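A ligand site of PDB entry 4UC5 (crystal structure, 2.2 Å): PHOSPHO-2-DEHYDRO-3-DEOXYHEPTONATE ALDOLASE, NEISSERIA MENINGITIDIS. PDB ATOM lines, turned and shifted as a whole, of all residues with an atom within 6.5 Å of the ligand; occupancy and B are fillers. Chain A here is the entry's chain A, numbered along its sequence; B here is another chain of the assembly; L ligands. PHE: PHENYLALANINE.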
ATOM      1  N   ARG A  42      -6.278   9.605 -29.575  1.00  0.00           N
ATOM      2  CA  ARG A  42      -6.282   8.134 -29.571  1.00  0.00           C
ATOM      3  C   ARG A  42      -6.048   7.557 -30.956  1.00  0.00           C
ATOM      4  O   ARG A  42      -5.242   6.643 -31.118  1.00  0.00           O
ATOM      5  CB  ARG A  42      -7.590   7.584 -29.025  1.00  0.00           C
ATOM      6  CG  ARG A  42      -7.690   7.750 -27.538  1.00  0.00           C
ATOM      7  CD  ARG A  42      -9.087   7.458 -27.055  1.00  0.00           C
ATOM      8  NE  ARG A  42      -9.203   7.670 -25.623  1.00  0.00           N
ATOM      9  CZ  ARG A  42     -10.358   7.624 -24.957  1.00  0.00           C
ATOM     10  NH1 ARG A  42     -11.483   7.402 -25.604  1.00  0.00           N
ATOM     11  NH2 ARG A  42     -10.385   7.830 -23.649  1.00  0.00           N
ATOM     12  N   PHE A 146      -3.071   3.587 -14.775  1.00  0.00           N
ATOM     13  CA  PHE A 146      -4.187   3.057 -14.039  1.00  0.00           C
ATOM     14  C   PHE A 146      -3.701   1.979 -13.065  1.00  0.00           C
ATOM     15  O   PHE A 146      -3.259   0.927 -13.482  1.00  0.00           O
ATOM     16  CB  PHE A 146      -5.189   2.512 -15.036  1.00  0.00           C
ATOM     17  CG  PHE A 146      -5.848   3.566 -15.887  1.00  0.00           C
ATOM     18  CD1 PHE A 146      -6.724   4.487 -15.333  1.00  0.00           C
ATOM     19  CD2 PHE A 146      -5.587   3.639 -17.252  1.00  0.00           C
ATOM     20  CE1 PHE A 146      -7.350   5.444 -16.116  1.00  0.00           C
ATOM     21  CE2 PHE A 146      -6.191   4.602 -18.044  1.00  0.00           C
ATOM     22  CZ  PHE A 146      -7.101   5.487 -17.484  1.00  0.00           C
ATOM     23  N   MET A 149      -8.800  -1.083 -10.841  1.00  0.00           N
ATOM     24  CA  MET A 149      -9.848  -1.375 -11.803  1.00  0.00           C
ATOM     25  C   MET A 149     -11.106  -0.486 -11.644  1.00  0.00           C
ATOM     26  O   MET A 149     -12.031  -0.569 -12.443  1.00  0.00           O
ATOM     27  CB  MET A 149     -10.210  -2.880 -11.696  1.00  0.00           C
ATOM     28  CG  MET A 149      -9.366  -3.835 -12.567  1.00  0.00           C
ATOM     29  SD  MET A 149      -7.567  -3.740 -12.341  1.00  0.00           S
ATOM     30  CE  MET A 149      -7.491  -4.187 -10.623  1.00  0.00           C
ATOM     31  N   ILE A 150     -11.108   0.344 -10.603  1.00  0.00           N
ATOM     32  CA  ILE A 150     -12.218   1.260 -10.325  1.00  0.00           C
ATOM     33  C   ILE A 150     -12.017   2.725 -10.756  1.00  0.00           C
ATOM     34  O   ILE A 150     -12.926   3.331 -11.302  1.00  0.00           O
ATOM     35  CB  ILE A 150     -12.633   1.191  -8.841  1.00  0.00           C
ATOM     36  CG1 ILE A 150     -13.093  -0.220  -8.486  1.00  0.00           C
ATOM     37  CG2 ILE A 150     -13.731   2.199  -8.546  1.00  0.00           C
ATOM     38  CD1 ILE A 150     -13.258  -0.453  -7.006  1.00  0.00           C
ATOM     39  N   PRO A 152     -10.495   4.117 -13.219  1.00  0.00           N
ATOM     40  CA  PRO A 152     -10.789   4.480 -14.606  1.00  0.00           C
ATOM     41  C   PRO A 152     -12.234   4.933 -14.881  1.00  0.00           C
ATOM     42  O   PRO A 152     -12.432   5.742 -15.768  1.00  0.00           O
ATOM     43  CB  PRO A 152     -10.522   3.183 -15.380  1.00  0.00           C
ATOM     44  CG  PRO A 152      -9.536   2.462 -14.537  1.00  0.00           C
ATOM     45  CD  PRO A 152      -9.970   2.752 -13.132  1.00  0.00           C
ATOM     46  N   GLN A 153     -13.204   4.426 -14.138  1.00  0.00           N
ATOM     47  CA  GLN A 153     -14.597   4.830 -14.351  1.00  0.00           C
ATOM     48  C   GLN A 153     -14.843   6.303 -14.020  1.00  0.00           C
ATOM     49  O   GLN A 153     -15.845   6.889 -14.411  1.00  0.00           O
ATOM     50  CB  GLN A 153     -15.541   3.956 -13.509  1.00  0.00           C
ATOM     51  CG  GLN A 153     -15.712   2.541 -14.040  1.00  0.00           C
ATOM     52  CD  GLN A 153     -16.516   2.473 -15.329  1.00  0.00           C
ATOM     53  OE1 GLN A 153     -16.104   3.005 -16.354  1.00  0.00           O
ATOM     54  NE2 GLN A 153     -17.663   1.812 -15.274  1.00  0.00           N
ATOM     55  N   ALA A 156     -11.380   8.032 -17.118  1.00  0.00           N
ATOM     56  CA  ALA A 156     -10.772   7.386 -18.274  1.00  0.00           C
ATOM     57  C   ALA A 156     -11.190   8.050 -19.571  1.00  0.00           C
ATOM     58  O   ALA A 156     -10.440   8.092 -20.521  1.00  0.00           O
ATOM     59  CB  ALA A 156     -11.084   5.910 -18.293  1.00  0.00           C
ATOM     60  N   ASP A 157     -12.421   8.516 -19.605  1.00  0.00           N
ATOM     61  CA  ASP A 157     -12.952   9.168 -20.783  1.00  0.00           C
ATOM     62  C   ASP A 157     -12.090  10.343 -21.245  1.00  0.00           C
ATOM     63  O   ASP A 157     -12.178  10.770 -22.398  1.00  0.00           O
ATOM     64  CB  ASP A 157     -14.386   9.624 -20.531  1.00  0.00           C
ATOM     65  CG  ASP A 157     -14.534  10.503 -19.320  1.00  0.00           C
ATOM     66  OD1 ASP A 157     -13.985  10.174 -18.217  1.00  0.00           O
ATOM     67  OD2 ASP A 157     -15.270  11.513 -19.464  1.00  0.00           O
ATOM     68  N   LEU A 177      -8.070  -5.327 -17.478  1.00  0.00           N
ATOM     69  CA  LEU A 177      -8.409  -3.908 -17.515  1.00  0.00           C
ATOM     70  C   LEU A 177      -8.007  -3.293 -18.863  1.00  0.00           C
ATOM     71  O   LEU A 177      -8.813  -2.636 -19.548  1.00  0.00           O
ATOM     72  CB  LEU A 177      -7.672  -3.164 -16.411  1.00  0.00           C
ATOM     73  CG  LEU A 177      -7.832  -1.635 -16.445  1.00  0.00           C
ATOM     74  CD1 LEU A 177      -9.308  -1.269 -16.309  1.00  0.00           C
ATOM     75  CD2 LEU A 177      -6.971  -0.981 -15.370  1.00  0.00           C
ATOM     76  N   GLY A 180     -10.019  -3.444 -21.975  1.00  0.00           N
ATOM     77  CA  GLY A 180     -11.260  -2.664 -22.025  1.00  0.00           C
ATOM     78  C   GLY A 180     -11.094  -1.159 -21.925  1.00  0.00           C
ATOM     79  O   GLY A 180     -12.082  -0.423 -21.907  1.00  0.00           O
ATOM     80  N   LEU A 181      -9.855  -0.682 -21.889  1.00  0.00           N
ATOM     81  CA  LEU A 181      -9.591   0.759 -21.878  1.00  0.00           C
ATOM     82  C   LEU A 181      -9.740   1.359 -23.255  1.00  0.00           C
ATOM     83  O   LEU A 181      -9.342   0.780 -24.248  1.00  0.00           O
ATOM     84  CB  LEU A 181      -8.210   1.054 -21.370  1.00  0.00           C
ATOM     85  CG  LEU A 181      -8.039   0.822 -19.866  1.00  0.00           C
ATOM     86  CD1 LEU A 181      -6.580   0.908 -19.485  1.00  0.00           C
ATOM     87  CD2 LEU A 181      -8.858   1.818 -19.051  1.00  0.00           C
ATOM     88  N   SER A 182     -10.307   2.562 -23.301  1.00  0.00           N
ATOM     89  CA  SER A 182     -10.655   3.202 -24.555  1.00  0.00           C
ATOM     90  C   SER A 182      -9.420   3.762 -25.256  1.00  0.00           C
ATOM     91  O   SER A 182      -9.403   3.966 -26.464  1.00  0.00           O
ATOM     92  CB  SER A 182     -11.677   4.308 -24.295  1.00  0.00           C
ATOM     93  OG  SER A 182     -12.882   3.785 -23.756  1.00  0.00           O
ATOM     94  N   CYS A 183      -8.372   3.979 -24.485  1.00  0.00           N
ATOM     95  CA  CYS A 183      -7.166   4.505 -24.996  1.00  0.00           C
ATOM     96  C   CYS A 183      -6.196   3.400 -25.389  1.00  0.00           C
ATOM     97  O   CYS A 183      -6.326   2.265 -24.929  1.00  0.00           O
ATOM     98  CB  CYS A 183      -6.541   5.380 -23.932  1.00  0.00           C
ATOM     99  SG  CYS A 183      -6.210   4.555 -22.384  1.00  0.00           S
ATOM    100  N   PHE A 211     -13.679  -8.608 -16.144  1.00  0.00           N
ATOM    101  CA  PHE A 211     -13.164  -8.237 -14.838  1.00  0.00           C
ATOM    102  C   PHE A 211     -14.220  -7.542 -13.993  1.00  0.00           C
ATOM    103  O   PHE A 211     -15.137  -6.943 -14.518  1.00  0.00           O
ATOM    104  CB  PHE A 211     -11.883  -7.415 -14.931  1.00  0.00           C
ATOM    105  CG  PHE A 211     -12.075  -6.050 -15.500  1.00  0.00           C
ATOM    106  CD1 PHE A 211     -11.967  -5.835 -16.862  1.00  0.00           C
ATOM    107  CD2 PHE A 211     -12.341  -4.971 -14.686  1.00  0.00           C
ATOM    108  CE1 PHE A 211     -12.137  -4.579 -17.384  1.00  0.00           C
ATOM    109  CE2 PHE A 211     -12.504  -3.716 -15.215  1.00  0.00           C
ATOM    110  CZ  PHE A 211     -12.405  -3.520 -16.567  1.00  0.00           C
ATOM    111  N   LEU A 212     -14.089  -7.660 -12.680  1.00  0.00           N
ATOM    112  CA  LEU A 212     -14.975  -6.985 -11.739  1.00  0.00           C
ATOM    113  C   LEU A 212     -14.632  -5.514 -11.563  1.00  0.00           C
ATOM    114  O   LEU A 212     -13.478  -5.131 -11.556  1.00  0.00           O
ATOM    115  CB  LEU A 212     -14.976  -7.702 -10.392  1.00  0.00           C
ATOM    116  CG  LEU A 212     -15.263  -9.210 -10.395  1.00  0.00           C
ATOM    117  CD1 LEU A 212     -15.918  -9.669  -9.113  1.00  0.00           C
ATOM    118  CD2 LEU A 212     -16.095  -9.618 -11.586  1.00  0.00           C
ATOM    119  N   SER A 213     -15.675  -4.705 -11.502  1.00  0.00           N
ATOM    120  CA  SER A 213     -15.573  -3.257 -11.436  1.00  0.00           C
ATOM    121  C   SER A 213     -16.937  -2.723 -11.053  1.00  0.00           C
ATOM    122  O   SER A 213     -17.849  -3.483 -10.739  1.00  0.00           O
ATOM    123  CB  SER A 213     -15.119  -2.679 -12.782  1.00  0.00           C
ATOM    124  OG  SER A 213     -14.604  -1.371 -12.600  1.00  0.00           O
ATOM    125  N   VAL A 214     -17.067  -1.405 -11.035  1.00  0.00           N
ATOM    126  CA  VAL A 214     -18.344  -0.791 -10.743  1.00  0.00           C
ATOM    127  C   VAL A 214     -18.900  -0.102 -11.982  1.00  0.00           C
ATOM    128  O   VAL A 214     -18.170   0.275 -12.864  1.00  0.00           O
ATOM    129  CB  VAL A 214     -18.270   0.225  -9.592  1.00  0.00           C
ATOM    130  CG1 VAL A 214     -17.729  -0.419  -8.337  1.00  0.00           C
ATOM    131  CG2 VAL A 214     -17.424   1.430  -9.993  1.00  0.00           C
ATOM    132  N   LYS A 216     -21.151   3.069 -13.764  1.00  0.00           N
ATOM    133  CA  LYS A 216     -21.076   4.509 -13.539  1.00  0.00           C
ATOM    134  C   LYS A 216     -21.851   4.892 -12.297  1.00  0.00           C
ATOM    135  O   LYS A 216     -21.500   5.855 -11.626  1.00  0.00           O
ATOM    136  CB  LYS A 216     -21.584   5.288 -14.740  1.00  0.00           C
ATOM    137  CG  LYS A 216     -20.702   5.229 -15.961  1.00  0.00           C
ATOM    138  CD  LYS A 216     -19.218   5.296 -15.622  1.00  0.00           C
ATOM    139  CE  LYS A 216     -18.374   5.614 -16.872  1.00  0.00           C
ATOM    140  NZ  LYS A 216     -18.037   4.423 -17.703  1.00  0.00           N
ATOM    141  N   VAL A 223     -17.527  -6.603 -16.092  1.00  0.00           N
ATOM    142  CA  VAL A 223     -17.181  -5.893 -17.308  1.00  0.00           C
ATOM    143  C   VAL A 223     -16.683  -6.848 -18.366  1.00  0.00           C
ATOM    144  O   VAL A 223     -15.689  -7.525 -18.141  1.00  0.00           O
ATOM    145  CB  VAL A 223     -16.064  -4.894 -17.038  1.00  0.00           C
ATOM    146  CG1 VAL A 223     -15.738  -4.106 -18.305  1.00  0.00           C
ATOM    147  CG2 VAL A 223     -16.458  -3.972 -15.902  1.00  0.00           C
ATOM    148  N   THR B   7     -16.051   9.007 -26.150  1.00  0.00           N
ATOM    149  CA  THR B   7     -14.775   8.680 -25.521  1.00  0.00           C
ATOM    150  C   THR B   7     -14.859   7.642 -24.397  1.00  0.00           C
ATOM    151  O   THR B   7     -13.845   7.236 -23.856  1.00  0.00           O
ATOM    152  CB  THR B   7     -14.096   9.942 -24.975  1.00  0.00           C
ATOM    153  OG1 THR B   7     -14.935  10.536 -23.984  1.00  0.00           O
ATOM    154  CG2 THR B   7     -13.855  10.933 -26.078  1.00  0.00           C
ATOM    155  N   ASP B   8     -16.065   7.240 -24.029  1.00  0.00           N
ATOM    156  CA  ASP B   8     -16.316   6.390 -22.871  1.00  0.00           C
ATOM    157  C   ASP B   8     -16.743   5.025 -23.335  1.00  0.00           C
ATOM    158  O   ASP B   8     -17.554   4.904 -24.240  1.00  0.00           O
ATOM    159  CB  ASP B   8     -17.431   7.019 -22.038  1.00  0.00           C
ATOM    160  CG  ASP B   8     -17.829   6.183 -20.828  1.00  0.00           C
ATOM    161  OD1 ASP B   8     -16.951   5.687 -20.086  1.00  0.00           O
ATOM    162  OD2 ASP B   8     -19.047   6.048 -20.619  1.00  0.00           O
ATOM    163  N   ASP B   9     -16.171   3.996 -22.698  1.00  0.00           N
ATOM    164  CA  ASP B   9     -16.500   2.585 -22.946  1.00  0.00           C
ATOM    165  C   ASP B   9     -16.413   2.099 -24.408  1.00  0.00           C
ATOM    166  O   ASP B   9     -17.115   1.194 -24.810  1.00  0.00           O
ATOM    167  CB  ASP B   9     -17.883   2.277 -22.334  1.00  0.00           C
ATOM    168  CG  ASP B   9     -17.854   2.159 -20.796  1.00  0.00           C
ATOM    169  OD1 ASP B   9     -16.759   2.319 -20.190  1.00  0.00           O
ATOM    170  OD2 ASP B   9     -18.915   1.909 -20.202  1.00  0.00           O
ATOM    171  N   ILE B  10     -15.486   2.660 -25.163  1.00  0.00           N
ATOM    172  CA  ILE B  10     -15.301   2.369 -26.596  1.00  0.00           C
ATOM    173  C   ILE B  10     -15.047   0.897 -26.906  1.00  0.00           C
ATOM    174  O   ILE B  10     -15.478   0.366 -27.940  1.00  0.00           O
ATOM    175  CB  ILE B  10     -14.096   3.176 -27.133  1.00  0.00           C
ATOM    176  CG1 ILE B  10     -14.326   4.682 -26.934  1.00  0.00           C
ATOM    177  CG2 ILE B  10     -13.800   2.868 -28.581  1.00  0.00           C
ATOM    178  CD1 ILE B  10     -15.574   5.223 -27.603  1.00  0.00           C
ATOM    179  N   LYS B  11     -14.320   0.266 -26.008  1.00  0.00           N
ATOM    180  CA  LYS B  11     -13.878  -1.105 -26.138  1.00  0.00           C
ATOM    181  C   LYS B  11     -14.558  -2.046 -25.154  1.00  0.00           C
ATOM    182  O   LYS B  11     -14.040  -3.109 -24.853  1.00  0.00           O
ATOM    183  CB  LYS B  11     -12.353  -1.182 -26.018  1.00  0.00           C
ATOM    184  CG  LYS B  11     -11.650  -0.332 -27.056  1.00  0.00           C
ATOM    185  CD  LYS B  11     -10.148  -0.378 -26.882  1.00  0.00           C
ATOM    186  CE  LYS B  11      -9.467   0.573 -27.853  1.00  0.00           C
ATOM    187  NZ  LYS B  11      -8.349   1.302 -27.223  1.00  0.00           N
ATOM    188  N   ILE B  12     -15.691  -1.624 -24.624  1.00  0.00           N
ATOM    189  CA  ILE B  12     -16.469  -2.436 -23.695  1.00  0.00           C
ATOM    190  C   ILE B  12     -17.665  -3.030 -24.459  1.00  0.00           C
ATOM    191  O   ILE B  12     -18.387  -2.324 -25.159  1.00  0.00           O
ATOM    192  CB  ILE B  12     -16.970  -1.578 -22.518  1.00  0.00           C
ATOM    193  CG1 ILE B  12     -15.782  -0.999 -21.717  1.00  0.00           C
ATOM    194  CG2 ILE B  12     -17.937  -2.352 -21.637  1.00  0.00           C
ATOM    195  CD1 ILE B  12     -14.789  -2.012 -21.174  1.00  0.00           C
ATOM    196  N   VAL B  15     -21.410  -3.833 -19.587  1.00  0.00           N
ATOM    197  CA  VAL B  15     -21.191  -3.725 -18.161  1.00  0.00           C
ATOM    198  C   VAL B  15     -22.494  -4.041 -17.444  1.00  0.00           C
ATOM    199  O   VAL B  15     -23.446  -3.277 -17.580  1.00  0.00           O
ATOM    200  CB  VAL B  15     -20.758  -2.315 -17.731  1.00  0.00           C
ATOM    201  CG1 VAL B  15     -20.567  -2.274 -16.218  1.00  0.00           C
ATOM    202  CG2 VAL B  15     -19.479  -1.912 -18.422  1.00  0.00           C
HETATM  203  N   PHE L   1     -14.639   3.333 -18.696  1.00  0.00           N
HETATM  204  CA  PHE L   1     -13.312   2.847 -19.140  1.00  0.00           C
HETATM  205  C   PHE L   1     -12.916   3.465 -20.468  1.00  0.00           C
HETATM  206  O   PHE L   1     -11.771   3.339 -20.892  1.00  0.00           O
HETATM  207  CB  PHE L   1     -13.309   1.339 -19.260  1.00  0.00           C
HETATM  208  CG  PHE L   1     -13.722   0.653 -18.002  1.00  0.00           C
HETATM  209  CD1 PHE L   1     -12.811   0.430 -16.988  1.00  0.00           C
HETATM  210  CD2 PHE L   1     -15.038   0.264 -17.810  1.00  0.00           C
HETATM  211  CE1 PHE L   1     -13.196  -0.190 -15.818  1.00  0.00           C
HETATM  212  CE2 PHE L   1     -15.428  -0.344 -16.634  1.00  0.00           C
HETATM  213  CZ  PHE L   1     -14.495  -0.561 -15.629  1.00  0.00           C
HETATM  214  OXT PHE L   1     -13.732   4.096 -21.127  1.00  0.00           O
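Residues that only touch the ligand: Ser 213 (3.1 Å), Gly 180 (3.4 Å), Phe 211 (3.5 Å), Leu 181 (3.5 Å), Met 149 (3.6 Å), Lys 216 (3.7 Å), Ala 156 (3.7 Å), Val 223 (3.8 Å), Pro 152 (3.9 Å) and Leu 177 (3.95 Å). Hydrophobic or aromatic side chains within 4 Å of the ligand: Pro 152, Ala 156, Leu 177, Leu 181, Phe 211 and Val 223. Within 4 Å of the ligand: Met 149, Pro 152, Gln 153, Ala 156, Leu 177, Gly 180, Leu 181, Ser 182, Phe 211, Ser 213, Lys 216, Val 223, Asp 8 of chain B and Asp 9 of chain B. The nearest printed residue that does not touch the ligand is Ile 12 of chain B (4.1 Å).
The backbone NH (N) of Asp 9 of chain B is in hydrogen-bond range of the side-chain hydroxyl (OG) of Ser 182 (3.5 Å). The backbone NH (N) of Ile 10 of chain B is in hydrogen-bond range of the side-chain hydroxyl (OG) of Ser 182. The backbone carbonyl oxygen (O) of Ser 182 sits at hydrogen-bond distance from the side-chain amino group (NZ) of Lys 11 of chain B (3.0 Å). NE2 of Gln 153 is in hydrogen-bond range of O of Val 214 (2.9 Å). The side-chain carboxylate of Asp 9 of chain B lies within salt-bridge range of the side-chain amino group of Lys 216 (3.5 Å). OG of Ser 213 sits at hydrogen-bond distance from O of Met 149. NZ of Lys 11 of chain B sits close to O of Leu 181, 3.2 Å away. The backbone carbonyl oxygen (O) of Ala 156 lies within hydrogen-bond range of the guanidinium group (NH2) of Arg 42, 3.1 Å away.
N of Ser 182 is in hydrogen-bond range of O of the ligand (2.9 Å). OG of Ser 182 sits at hydrogen-bond distance from OXT of the ligand (2.8 Å). OE1 of Gln 153 is in hydrogen-bond range of N of the ligand (2.8 Å). The backbone NH (N) of Asp 9 of chain B is in hydrogen-bond range of an oxygen (OXT) of the ligand (2.9 Å). The side-chain carboxylate (OD1) of Asp 9 of chain B is in salt-bridge range of a nitrogen (N) of the ligand, 2.8 Å away. A nitrogen (N) of the ligand is in salt-bridge range of the side-chain carboxylate (OD1) of Asp 8 of chain B, 3.6 Å away.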
